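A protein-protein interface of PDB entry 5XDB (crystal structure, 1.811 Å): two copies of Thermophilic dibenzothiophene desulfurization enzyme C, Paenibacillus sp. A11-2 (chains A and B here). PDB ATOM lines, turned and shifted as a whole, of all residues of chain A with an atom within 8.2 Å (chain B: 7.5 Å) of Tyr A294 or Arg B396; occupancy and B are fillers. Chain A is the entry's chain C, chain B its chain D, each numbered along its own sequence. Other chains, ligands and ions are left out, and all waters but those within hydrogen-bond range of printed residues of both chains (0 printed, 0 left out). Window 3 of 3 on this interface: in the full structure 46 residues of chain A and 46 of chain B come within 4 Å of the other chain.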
ATOM      1  N   PHE A 281     -30.529  10.966  -4.154  1.00  0.00           N
ATOM      2  CA  PHE A 281     -30.374  12.012  -3.141  1.00  0.00           C
ATOM      3  C   PHE A 281     -31.690  12.782  -3.041  1.00  0.00           C
ATOM      4  O   PHE A 281     -31.839  13.913  -3.513  1.00  0.00           O
ATOM      5  CB  PHE A 281     -29.204  12.928  -3.474  1.00  0.00           C
ATOM      6  CG  PHE A 281     -28.777  13.796  -2.320  1.00  0.00           C
ATOM      7  CD1 PHE A 281     -28.373  13.226  -1.122  1.00  0.00           C
ATOM      8  CD2 PHE A 281     -28.779  15.175  -2.428  1.00  0.00           C
ATOM      9  CE1 PHE A 281     -27.977  14.016  -0.065  1.00  0.00           C
ATOM     10  CE2 PHE A 281     -28.375  15.968  -1.365  1.00  0.00           C
ATOM     11  CZ  PHE A 281     -27.975  15.392  -0.192  1.00  0.00           C
ATOM     12  N   LEU A 283     -33.079  14.388  -0.811  1.00  0.00           N
ATOM     13  CA  LEU A 283     -33.020  15.737  -0.261  1.00  0.00           C
ATOM     14  C   LEU A 283     -33.077  16.796  -1.352  1.00  0.00           C
ATOM     15  O   LEU A 283     -33.565  17.905  -1.111  1.00  0.00           O
ATOM     16  CB  LEU A 283     -31.754  15.911   0.566  1.00  0.00           C
ATOM     17  CG  LEU A 283     -32.006  15.784   2.063  1.00  0.00           C
ATOM     18  CD1 LEU A 283     -30.843  15.083   2.718  1.00  0.00           C
ATOM     19  CD2 LEU A 283     -32.212  17.159   2.664  1.00  0.00           C
ATOM     20  N   ALA A 284     -32.578  16.480  -2.548  1.00  0.00           N
ATOM     21  CA  ALA A 284     -32.588  17.411  -3.665  1.00  0.00           C
ATOM     22  C   ALA A 284     -33.698  17.112  -4.665  1.00  0.00           C
ATOM     23  O   ALA A 284     -33.714  17.701  -5.751  1.00  0.00           O
ATOM     24  CB  ALA A 284     -31.230  17.408  -4.374  1.00  0.00           C
ATOM     25  N   VAL A 286     -34.262  14.158  -6.177  1.00  0.00           N
ATOM     26  CA  VAL A 286     -33.935  13.109  -7.135  1.00  0.00           C
ATOM     27  C   VAL A 286     -34.728  11.856  -6.793  1.00  0.00           C
ATOM     28  O   VAL A 286     -34.798  11.449  -5.624  1.00  0.00           O
ATOM     29  CB  VAL A 286     -32.421  12.828  -7.132  1.00  0.00           C
ATOM     30  CG1 VAL A 286     -32.093  11.659  -8.048  1.00  0.00           C
ATOM     31  CG2 VAL A 286     -31.655  14.080  -7.533  1.00  0.00           C
ATOM     32  N   ALA A 289     -31.088   7.478  -8.836  1.00  0.00           N
ATOM     33  CA  ALA A 289     -29.691   7.882  -8.947  1.00  0.00           C
ATOM     34  C   ALA A 289     -29.234   7.907 -10.399  1.00  0.00           C
ATOM     35  O   ALA A 289     -28.387   8.725 -10.773  1.00  0.00           O
ATOM     36  CB  ALA A 289     -28.809   6.935  -8.127  1.00  0.00           C
ATOM     37  N   GLU A 291     -30.802   8.970 -12.864  1.00  0.00           N
ATOM     38  CA  GLU A 291     -31.251  10.211 -13.480  1.00  0.00           C
ATOM     39  C   GLU A 291     -30.638  11.441 -12.821  1.00  0.00           C
ATOM     40  O   GLU A 291     -30.960  12.572 -13.208  1.00  0.00           O
ATOM     41  CB  GLU A 291     -32.784  10.308 -13.435  1.00  0.00           C
ATOM     42  CG  GLU A 291     -33.490   9.199 -14.204  1.00  0.00           C
ATOM     43  CD  GLU A 291     -33.156   9.207 -15.701  1.00  0.00           C
ATOM     44  OE1 GLU A 291     -33.044  10.305 -16.300  1.00  0.00           O
ATOM     45  OE2 GLU A 291     -33.005   8.109 -16.283  1.00  0.00           O
ATOM     46  N   ASP A 292     -29.760  11.254 -11.850  1.00  0.00           N
ATOM     47  CA  ASP A 292     -29.130  12.390 -11.192  1.00  0.00           C
ATOM     48  C   ASP A 292     -28.219  13.122 -12.172  1.00  0.00           C
ATOM     49  O   ASP A 292     -27.378  12.486 -12.809  1.00  0.00           O
ATOM     50  CB  ASP A 292     -28.333  11.902  -9.990  1.00  0.00           C
ATOM     51  CG  ASP A 292     -27.675  13.040  -9.233  1.00  0.00           C
ATOM     52  OD1 ASP A 292     -26.668  13.592  -9.727  1.00  0.00           O
ATOM     53  OD2 ASP A 292     -28.182  13.387  -8.151  1.00  0.00           O
ATOM     54  N   PRO A 293     -28.339  14.450 -12.309  1.00  0.00           N
ATOM     55  CA  PRO A 293     -27.538  15.151 -13.333  1.00  0.00           C
ATOM     56  C   PRO A 293     -26.044  15.095 -13.077  1.00  0.00           C
ATOM     57  O   PRO A 293     -25.252  15.109 -14.027  1.00  0.00           O
ATOM     58  CB  PRO A 293     -28.055  16.592 -13.262  1.00  0.00           C
ATOM     59  CG  PRO A 293     -28.600  16.724 -11.850  1.00  0.00           C
ATOM     60  CD  PRO A 293     -29.172  15.374 -11.517  1.00  0.00           C
ATOM     61  N   TYR A 294     -25.637  15.019 -11.817  1.00  0.00           N
ATOM     62  CA  TYR A 294     -24.217  14.980 -11.492  1.00  0.00           C
ATOM     63  C   TYR A 294     -23.652  13.566 -11.596  1.00  0.00           C
ATOM     64  O   TYR A 294     -22.505  13.396 -12.024  1.00  0.00           O
ATOM     65  CB  TYR A 294     -24.014  15.590 -10.101  1.00  0.00           C
ATOM     66  CG  TYR A 294     -24.657  16.968 -10.033  1.00  0.00           C
ATOM     67  CD1 TYR A 294     -24.385  17.917 -11.002  1.00  0.00           C
ATOM     68  CD2 TYR A 294     -25.572  17.291  -9.039  1.00  0.00           C
ATOM     69  CE1 TYR A 294     -24.972  19.169 -10.970  1.00  0.00           C
ATOM     70  CE2 TYR A 294     -26.170  18.544  -8.995  1.00  0.00           C
ATOM     71  CZ  TYR A 294     -25.870  19.470  -9.975  1.00  0.00           C
ATOM     72  OH  TYR A 294     -26.456  20.722  -9.944  1.00  0.00           O
ATOM     73  N   VAL A 295     -24.437  12.542 -11.253  1.00  0.00           N
ATOM     74  CA  VAL A 295     -24.033  11.173 -11.569  1.00  0.00           C
ATOM     75  C   VAL A 295     -23.819  11.022 -13.071  1.00  0.00           C
ATOM     76  O   VAL A 295     -22.806  10.470 -13.525  1.00  0.00           O
ATOM     77  CB  VAL A 295     -25.077  10.166 -11.060  1.00  0.00           C
ATOM     78  CG1 VAL A 295     -24.772   8.775 -11.620  1.00  0.00           C
ATOM     79  CG2 VAL A 295     -25.104  10.144  -9.530  1.00  0.00           C
ATOM     80  N   LEU A 296     -24.783  11.501 -13.861  1.00  0.00           N
ATOM     81  CA  LEU A 296     -24.696  11.372 -15.312  1.00  0.00           C
ATOM     82  C   LEU A 296     -23.483  12.114 -15.864  1.00  0.00           C
ATOM     83  O   LEU A 296     -22.837  11.644 -16.809  1.00  0.00           O
ATOM     84  CB  LEU A 296     -25.991  11.875 -15.958  1.00  0.00           C
ATOM     85  CG  LEU A 296     -27.201  10.940 -15.807  1.00  0.00           C
ATOM     86  CD1 LEU A 296     -28.496  11.666 -16.239  1.00  0.00           C
ATOM     87  CD2 LEU A 296     -26.988   9.640 -16.604  1.00  0.00           C
ATOM     88  N   ALA A 297     -23.150  13.273 -15.283  1.00  0.00           N
ATOM     89  CA  ALA A 297     -21.999  14.038 -15.762  1.00  0.00           C
ATOM     90  C   ALA A 297     -20.678  13.318 -15.490  1.00  0.00           C
ATOM     91  O   ALA A 297     -19.749  13.392 -16.301  1.00  0.00           O
ATOM     92  CB  ALA A 297     -21.990  15.428 -15.118  1.00  0.00           C
ATOM     93  N   ILE A 298     -20.562  12.634 -14.346  1.00  0.00           N
ATOM     94  CA  ILE A 298     -19.349  11.867 -14.066  1.00  0.00           C
ATOM     95  C   ILE A 298     -19.166  10.755 -15.094  1.00  0.00           C
ATOM     96  O   ILE A 298     -18.094  10.611 -15.697  1.00  0.00           O
ATOM     97  CB  ILE A 298     -19.384  11.308 -12.632  1.00  0.00           C
ATOM     98  CG1 ILE A 298     -19.258  12.452 -11.622  1.00  0.00           C
ATOM     99  CG2 ILE A 298     -18.297  10.243 -12.437  1.00  0.00           C
ATOM    100  CD1 ILE A 298     -19.408  12.006 -10.172  1.00  0.00           C
ATOM    101  N   TYR A 299     -20.197   9.924 -15.289  1.00  0.00           N
ATOM    102  CA  TYR A 299     -20.097   8.883 -16.310  1.00  0.00           C
ATOM    103  C   TYR A 299     -19.823   9.479 -17.683  1.00  0.00           C
ATOM    104  O   TYR A 299     -19.027   8.929 -18.452  1.00  0.00           O
ATOM    105  CB  TYR A 299     -21.363   8.025 -16.340  1.00  0.00           C
ATOM    106  CG  TYR A 299     -21.361   7.052 -15.197  1.00  0.00           C
ATOM    107  CD1 TYR A 299     -20.482   5.970 -15.185  1.00  0.00           C
ATOM    108  CD2 TYR A 299     -22.203   7.230 -14.108  1.00  0.00           C
ATOM    109  CE1 TYR A 299     -20.447   5.092 -14.120  1.00  0.00           C
ATOM    110  CE2 TYR A 299     -22.178   6.343 -13.034  1.00  0.00           C
ATOM    111  CZ  TYR A 299     -21.302   5.283 -13.051  1.00  0.00           C
ATOM    112  OH  TYR A 299     -21.261   4.412 -11.991  1.00  0.00           O
ATOM    113  N   GLY A 300     -20.473  10.599 -18.005  1.00  0.00           N
ATOM    114  CA  GLY A 300     -20.294  11.203 -19.314  1.00  0.00           C
ATOM    115  C   GLY A 300     -18.872  11.681 -19.549  1.00  0.00           C
ATOM    116  O   GLY A 300     -18.287  11.441 -20.610  1.00  0.00           O
ATOM    117  N   GLU A 301     -18.308  12.396 -18.571  1.00  0.00           N
ATOM    118  CA  GLU A 301     -16.942  12.899 -18.710  1.00  0.00           C
ATOM    119  C   GLU A 301     -15.958  11.760 -18.928  1.00  0.00           C
ATOM    120  O   GLU A 301     -15.093  11.822 -19.812  1.00  0.00           O
ATOM    121  CB  GLU A 301     -16.547  13.691 -17.459  1.00  0.00           C
ATOM    122  CG  GLU A 301     -17.271  15.009 -17.282  1.00  0.00           C
ATOM    123  CD  GLU A 301     -16.442  16.199 -17.739  1.00  0.00           C
ATOM    124  OE1 GLU A 301     -15.477  16.001 -18.515  1.00  0.00           O
ATOM    125  OE2 GLU A 301     -16.758  17.334 -17.321  1.00  0.00           O
ATOM    126  N   ARG A 358     -12.510   9.003  -8.717  1.00  0.00           N
ATOM    127  CA  ARG A 358     -13.691   9.865  -8.738  1.00  0.00           C
ATOM    128  C   ARG A 358     -15.007   9.109  -8.957  1.00  0.00           C
ATOM    129  O   ARG A 358     -16.063   9.627  -8.583  1.00  0.00           O
ATOM    130  CB  ARG A 358     -13.535  10.942  -9.821  1.00  0.00           C
ATOM    131  CG  ARG A 358     -12.337  11.885  -9.636  1.00  0.00           C
ATOM    132  CD  ARG A 358     -12.638  13.122  -8.778  1.00  0.00           C
ATOM    133  NE  ARG A 358     -14.037  13.563  -8.847  1.00  0.00           N
ATOM    134  CZ  ARG A 358     -14.596  14.156  -9.899  1.00  0.00           C
ATOM    135  NH1 ARG A 358     -13.883  14.380 -11.000  1.00  0.00           N
ATOM    136  NH2 ARG A 358     -15.876  14.518  -9.857  1.00  0.00           N
ATOM    137  N   GLU A 361     -17.745   8.965  -6.317  1.00  0.00           N
ATOM    138  CA  GLU A 361     -18.722  10.049  -6.196  1.00  0.00           C
ATOM    139  C   GLU A 361     -19.993   9.785  -6.990  1.00  0.00           C
ATOM    140  O   GLU A 361     -21.039  10.353  -6.660  1.00  0.00           O
ATOM    141  CB  GLU A 361     -18.092  11.376  -6.637  1.00  0.00           C
ATOM    142  CG  GLU A 361     -16.897  11.740  -5.777  1.00  0.00           C
ATOM    143  CD  GLU A 361     -16.003  12.817  -6.376  1.00  0.00           C
ATOM    144  OE1 GLU A 361     -16.559  13.817  -6.888  1.00  0.00           O
ATOM    145  OE2 GLU A 361     -14.745  12.658  -6.313  1.00  0.00           O
ATOM    146  N   ALA A 362     -19.933   8.942  -8.027  1.00  0.00           N
ATOM    147  CA  ALA A 362     -21.129   8.514  -8.740  1.00  0.00           C
ATOM    148  C   ALA A 362     -21.818   7.316  -8.099  1.00  0.00           C
ATOM    149  O   ALA A 362     -22.932   6.967  -8.512  1.00  0.00           O
ATOM    150  CB  ALA A 362     -20.785   8.166 -10.193  1.00  0.00           C
ATOM    151  N   ILE B 346     -16.014  21.967   0.030  1.00  0.00           N
ATOM    152  CA  ILE B 346     -15.810  21.665  -1.381  1.00  0.00           C
ATOM    153  C   ILE B 346     -14.324  21.698  -1.710  1.00  0.00           C
ATOM    154  O   ILE B 346     -13.765  20.746  -2.266  1.00  0.00           O
ATOM    155  CB  ILE B 346     -16.604  22.661  -2.250  1.00  0.00           C
ATOM    156  CG1 ILE B 346     -18.114  22.438  -2.079  1.00  0.00           C
ATOM    157  CG2 ILE B 346     -16.195  22.534  -3.721  1.00  0.00           C
ATOM    158  CD1 ILE B 346     -18.974  23.647  -2.543  1.00  0.00           C
ATOM    159  N   PRO B 390     -23.027  14.137  -0.673  1.00  0.00           N
ATOM    160  CA  PRO B 390     -22.443  14.352  -2.010  1.00  0.00           C
ATOM    161  C   PRO B 390     -21.950  15.779  -2.205  1.00  0.00           C
ATOM    162  O   PRO B 390     -22.715  16.736  -2.072  1.00  0.00           O
ATOM    163  CB  PRO B 390     -23.605  14.022  -2.961  1.00  0.00           C
ATOM    164  CG  PRO B 390     -24.834  14.136  -2.114  1.00  0.00           C
ATOM    165  CD  PRO B 390     -24.439  13.728  -0.743  1.00  0.00           C
ATOM    166  N   VAL B 391     -20.666  15.915  -2.555  1.00  0.00           N
ATOM    167  CA  VAL B 391     -20.102  17.248  -2.758  1.00  0.00           C
ATOM    168  C   VAL B 391     -20.783  17.967  -3.920  1.00  0.00           C
ATOM    169  O   VAL B 391     -20.840  19.206  -3.945  1.00  0.00           O
ATOM    170  CB  VAL B 391     -18.567  17.162  -2.952  1.00  0.00           C
ATOM    171  CG1 VAL B 391     -18.205  16.547  -4.303  1.00  0.00           C
ATOM    172  CG2 VAL B 391     -17.925  18.541  -2.773  1.00  0.00           C
ATOM    173  N   ALA B 392     -21.316  17.212  -4.894  1.00  0.00           N
ATOM    174  CA  ALA B 392     -22.037  17.836  -6.006  1.00  0.00           C
ATOM    175  C   ALA B 392     -23.170  18.721  -5.506  1.00  0.00           C
ATOM    176  O   ALA B 392     -23.460  19.766  -6.100  1.00  0.00           O
ATOM    177  CB  ALA B 392     -22.599  16.768  -6.950  1.00  0.00           C
ATOM    178  N   TYR B 393     -23.828  18.319  -4.419  1.00  0.00           N
ATOM    179  CA  TYR B 393     -24.931  19.122  -3.911  1.00  0.00           C
ATOM    180  C   TYR B 393     -24.476  20.225  -2.971  1.00  0.00           C
ATOM    181  O   TYR B 393     -25.170  21.245  -2.869  1.00  0.00           O
ATOM    182  CB  TYR B 393     -25.995  18.211  -3.274  1.00  0.00           C
ATOM    183  CG  TYR B 393     -26.771  17.554  -4.398  1.00  0.00           C
ATOM    184  CD1 TYR B 393     -27.774  18.247  -5.072  1.00  0.00           C
ATOM    185  CD2 TYR B 393     -26.424  16.292  -4.867  1.00  0.00           C
ATOM    186  CE1 TYR B 393     -28.448  17.678  -6.142  1.00  0.00           C
ATOM    187  CE2 TYR B 393     -27.094  15.722  -5.928  1.00  0.00           C
ATOM    188  CZ  TYR B 393     -28.101  16.414  -6.559  1.00  0.00           C
ATOM    189  OH  TYR B 393     -28.762  15.841  -7.618  1.00  0.00           O
ATOM    190  N   LYS B 394     -23.308  20.092  -2.332  1.00  0.00           N
ATOM    191  CA  LYS B 394     -22.710  21.267  -1.700  1.00  0.00           C
ATOM    192  C   LYS B 394     -22.374  22.327  -2.745  1.00  0.00           C
ATOM    193  O   LYS B 394     -22.598  23.524  -2.533  1.00  0.00           O
ATOM    194  CB  LYS B 394     -21.458  20.875  -0.908  1.00  0.00           C
ATOM    195  CG  LYS B 394     -21.780  20.068   0.345  1.00  0.00           C
ATOM    196  CD  LYS B 394     -22.289  20.983   1.455  1.00  0.00           C
ATOM    197  CE  LYS B 394     -23.206  20.248   2.438  1.00  0.00           C
ATOM    198  NZ  LYS B 394     -24.496  19.848   1.812  1.00  0.00           N
ATOM    199  N   ILE B 395     -21.847  21.899  -3.890  1.00  0.00           N
ATOM    200  CA  ILE B 395     -21.564  22.824  -4.982  1.00  0.00           C
ATOM    201  C   ILE B 395     -22.854  23.478  -5.484  1.00  0.00           C
ATOM    202  O   ILE B 395     -22.918  24.700  -5.681  1.00  0.00           O
ATOM    203  CB  ILE B 395     -20.806  22.083  -6.102  1.00  0.00           C
ATOM    204  CG1 ILE B 395     -19.395  21.721  -5.612  1.00  0.00           C
ATOM    205  CG2 ILE B 395     -20.786  22.904  -7.390  1.00  0.00           C
ATOM    206  CD1 ILE B 395     -18.613  20.798  -6.559  1.00  0.00           C
ATOM    207  N   ARG B 396     -23.903  22.675  -5.701  1.00  0.00           N
ATOM    208  CA  ARG B 396     -25.177  23.253  -6.124  1.00  0.00           C
ATOM    209  C   ARG B 396     -25.679  24.259  -5.096  1.00  0.00           C
ATOM    210  O   ARG B 396     -26.207  25.322  -5.457  1.00  0.00           O
ATOM    211  CB  ARG B 396     -26.221  22.154  -6.353  1.00  0.00           C
ATOM    212  CG  ARG B 396     -27.509  22.697  -6.976  1.00  0.00           C
ATOM    213  CD  ARG B 396     -28.641  21.665  -7.007  1.00  0.00           C
ATOM    214  NE  ARG B 396     -29.746  22.143  -7.842  1.00  0.00           N
ATOM    215  CZ  ARG B 396     -30.682  22.997  -7.443  1.00  0.00           C
ATOM    216  NH1 ARG B 396     -30.672  23.488  -6.202  1.00  0.00           N
ATOM    217  NH2 ARG B 396     -31.638  23.373  -8.295  1.00  0.00           N
ATOM    218  N   GLU B 397     -25.514  23.949  -3.805  1.00  0.00           N
ATOM    219  CA  GLU B 397     -25.991  24.857  -2.768  1.00  0.00           C
ATOM    220  C   GLU B 397     -25.252  26.186  -2.826  1.00  0.00           C
ATOM    221  O   GLU B 397     -25.878  27.251  -2.745  1.00  0.00           O
ATOM    222  CB  GLU B 397     -25.853  24.202  -1.386  1.00  0.00           C
ATOM    223  CG  GLU B 397     -26.892  23.087  -1.177  1.00  0.00           C
ATOM    224  CD  GLU B 397     -26.474  22.001  -0.190  1.00  0.00           C
ATOM    225  OE1 GLU B 397     -25.466  22.162   0.533  1.00  0.00           O
ATOM    226  OE2 GLU B 397     -27.170  20.956  -0.140  1.00  0.00           O
ATOM    227  N   VAL B 398     -23.929  26.154  -3.003  1.00  0.00           N
ATOM    228  CA  VAL B 398     -23.189  27.407  -3.112  1.00  0.00           C
ATOM    229  C   VAL B 398     -23.588  28.154  -4.379  1.00  0.00           C
ATOM    230  O   VAL B 398     -23.707  29.386  -4.379  1.00  0.00           O
ATOM    231  CB  VAL B 398     -21.672  27.147  -3.047  1.00  0.00           C
ATOM    232  CG1 VAL B 398     -20.892  28.425  -3.337  1.00  0.00           C
ATOM    233  CG2 VAL B 398     -21.301  26.580  -1.674  1.00  0.00           C
ATOM    234  N   GLY B 399     -23.823  27.423  -5.473  1.00  0.00           N
ATOM    235  CA  GLY B 399     -24.227  28.071  -6.708  1.00  0.00           C
ATOM    236  C   GLY B 399     -25.607  28.693  -6.618  1.00  0.00           C
ATOM    237  O   GLY B 399     -25.841  29.779  -7.152  1.00  0.00           O
ATOM    238  N   ASN B 400     -26.539  28.006  -5.957  1.00  0.00           N
ATOM    239  CA  ASN B 400     -27.888  28.535  -5.784  1.00  0.00           C
ATOM    240  C   ASN B 400     -27.852  29.804  -4.936  1.00  0.00           C
ATOM    241  O   ASN B 400     -28.596  30.759  -5.194  1.00  0.00           O
ATOM    242  CB  ASN B 400     -28.766  27.457  -5.145  1.00  0.00           C
ATOM    243  CG  ASN B 400     -30.258  27.642  -5.424  1.00  0.00           C
ATOM    244  OD1 ASN B 400     -30.658  28.260  -6.411  1.00  0.00           O
ATOM    245  ND2 ASN B 400     -31.082  27.071  -4.555  1.00  0.00           N
ATOM    246  N   TRP B 401     -26.969  29.842  -3.934  1.00  0.00           N
ATOM    247  CA  TRP B 401     -26.785  31.069  -3.166  1.00  0.00           C
ATOM    248  C   TRP B 401     -26.210  32.179  -4.040  1.00  0.00           C
ATOM    249  O   TRP B 401     -26.756  33.284  -4.092  1.00  0.00           O
ATOM    250  CB  TRP B 401     -25.890  30.805  -1.953  1.00  0.00           C
ATOM    251  CG  TRP B 401     -25.317  32.054  -1.359  1.00  0.00           C
ATOM    252  CD1 TRP B 401     -25.952  32.947  -0.543  1.00  0.00           C
ATOM    253  CD2 TRP B 401     -23.987  32.541  -1.532  1.00  0.00           C
ATOM    254  NE1 TRP B 401     -25.092  33.964  -0.202  1.00  0.00           N
ATOM    255  CE2 TRP B 401     -23.882  33.741  -0.802  1.00  0.00           C
ATOM    256  CE3 TRP B 401     -22.873  32.085  -2.245  1.00  0.00           C
ATOM    257  CZ2 TRP B 401     -22.700  34.489  -0.759  1.00  0.00           C
ATOM    258  CZ3 TRP B 401     -21.704  32.829  -2.202  1.00  0.00           C
ATOM    259  CH2 TRP B 401     -21.627  34.010  -1.457  1.00  0.00           C
ATOM    260  N   PHE B 402     -25.116  31.901  -4.759  1.00  0.00           N
ATOM    261  CA  PHE B 402     -24.449  32.982  -5.478  1.00  0.00           C
ATOM    262  C   PHE B 402     -25.306  33.498  -6.622  1.00  0.00           C
ATOM    263  O   PHE B 402     -25.387  34.711  -6.847  1.00  0.00           O
ATOM    264  CB  PHE B 402     -23.089  32.544  -6.022  1.00  0.00           C
ATOM    265  CG  PHE B 402     -22.285  33.693  -6.558  1.00  0.00           C
ATOM    266  CD1 PHE B 402     -21.445  34.409  -5.723  1.00  0.00           C
ATOM    267  CD2 PHE B 402     -22.421  34.098  -7.881  1.00  0.00           C
ATOM    268  CE1 PHE B 402     -20.726  35.496  -6.208  1.00  0.00           C
ATOM    269  CE2 PHE B 402     -21.706  35.177  -8.372  1.00  0.00           C
ATOM    270  CZ  PHE B 402     -20.859  35.882  -7.540  1.00  0.00           C
ATOM    271  N   ASN B 404     -28.784  32.812  -7.304  1.00  0.00           N
ATOM    272  CA  ASN B 404     -30.192  33.088  -7.024  1.00  0.00           C
ATOM    273  C   ASN B 404     -30.444  33.689  -5.645  1.00  0.00           C
ATOM    274  O   ASN B 404     -31.607  33.911  -5.287  1.00  0.00           O
ATOM    275  CB  ASN B 404     -31.007  31.799  -7.191  1.00  0.00           C
ATOM    276  CG  ASN B 404     -30.964  31.282  -8.616  1.00  0.00           C
ATOM    277  OD1 ASN B 404     -31.139  32.053  -9.560  1.00  0.00           O
ATOM    278  ND2 ASN B 404     -30.703  29.987  -8.783  1.00  0.00           N
ATOM    279  N   ARG B 406     -30.315  32.377  -2.765  1.00  0.00           N
ATOM    280  CA  ARG B 406     -31.079  31.453  -1.933  1.00  0.00           C
ATOM    281  C   ARG B 406     -30.123  30.729  -0.998  1.00  0.00           C
ATOM    282  O   ARG B 406     -29.206  30.042  -1.461  1.00  0.00           O
ATOM    283  CB  ARG B 406     -31.851  30.441  -2.779  1.00  0.00           C
ATOM    284  CG  ARG B 406     -32.993  31.034  -3.601  1.00  0.00           C
ATOM    285  CD  ARG B 406     -33.844  29.924  -4.217  1.00  0.00           C
ATOM    286  NE  ARG B 406     -35.158  30.396  -4.655  1.00  0.00           N
ATOM    287  CZ  ARG B 406     -35.458  30.738  -5.905  1.00  0.00           C
ATOM    288  NH1 ARG B 406     -34.537  30.664  -6.860  1.00  0.00           N
ATOM    289  NH2 ARG B 406     -36.684  31.154  -6.201  1.00  0.00           N
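Of the printed residues of chain B, Val A286 touches Tyr B393 (3.4 Å).
Printed residues of chain B within 4 Å of Pro A293: Tyr B393 (3.9 Å).
Of the printed residues of chain B, Tyr A294 touches Ala B392 (3.6 Å), Tyr B393 (3.6 Å) and Arg B396 (3.7 Å).
Printed residues of chain A within 4 Å of Pro B390: Phe A281 (3.6 Å).
Lys B394 touches none of the printed residues of chain A.
Of the printed residues of chain A, Arg B396 touches Tyr A294.
Glu B397 touches none of the printed residues of chain A.
The nearest residue of chain A that does not touch Arg B396 is Ala A284 (5.6 Å).
The nearest printed residue of chain A that does not touch Pro B390 is Glu A361 (5.8 Å).
Of the 16 printed residues of chain B, 4 touch a printed residue of chain A.
Hydrophobic or aromatic side chains of chain B that line the printed part of chain A: Pro B390, Ala B392 and Tyr B393.
Of the 19 printed residues of chain A, 6 touch a printed residue of chain B.
Hydrophobic or aromatic side chains of chain A that line the printed part of chain B: Phe A281, Ala A284, Val A286, Pro A293 and Tyr A294.
Among the printed residues, 9 pairs touch across the chains.
Among the printed residues, no Asp or Glu carboxylate lies within 4 Å of a Lys or Arg side-chain nitrogen of the other chain.
N of Val A295 is in hydrogen-bond range of OD1 of Asp A292, at 2.9 Å.
The backbone NH of Tyr A294 sits at hydrogen-bond distance from the side-chain carboxylate of Asp A292, 2.7 Å away.
The side-chain carboxylate (OD2) of Asp A292 lies within hydrogen-bond range of the side-chain hydroxyl (OH) of Tyr B393 (2.6 Å).
No position is printed for both chains.
Among the printed residues, merely in contact across the chains: Ala A284 with Tyr B393, Val A286 with Tyr B393, Phe A281 with Tyr B393, Phe A281 with Pro B390, Tyr A294 with Tyr B393, Tyr A294 with Ala B392, Tyr A294 with Arg B396 and Pro A293 with Tyr B393.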
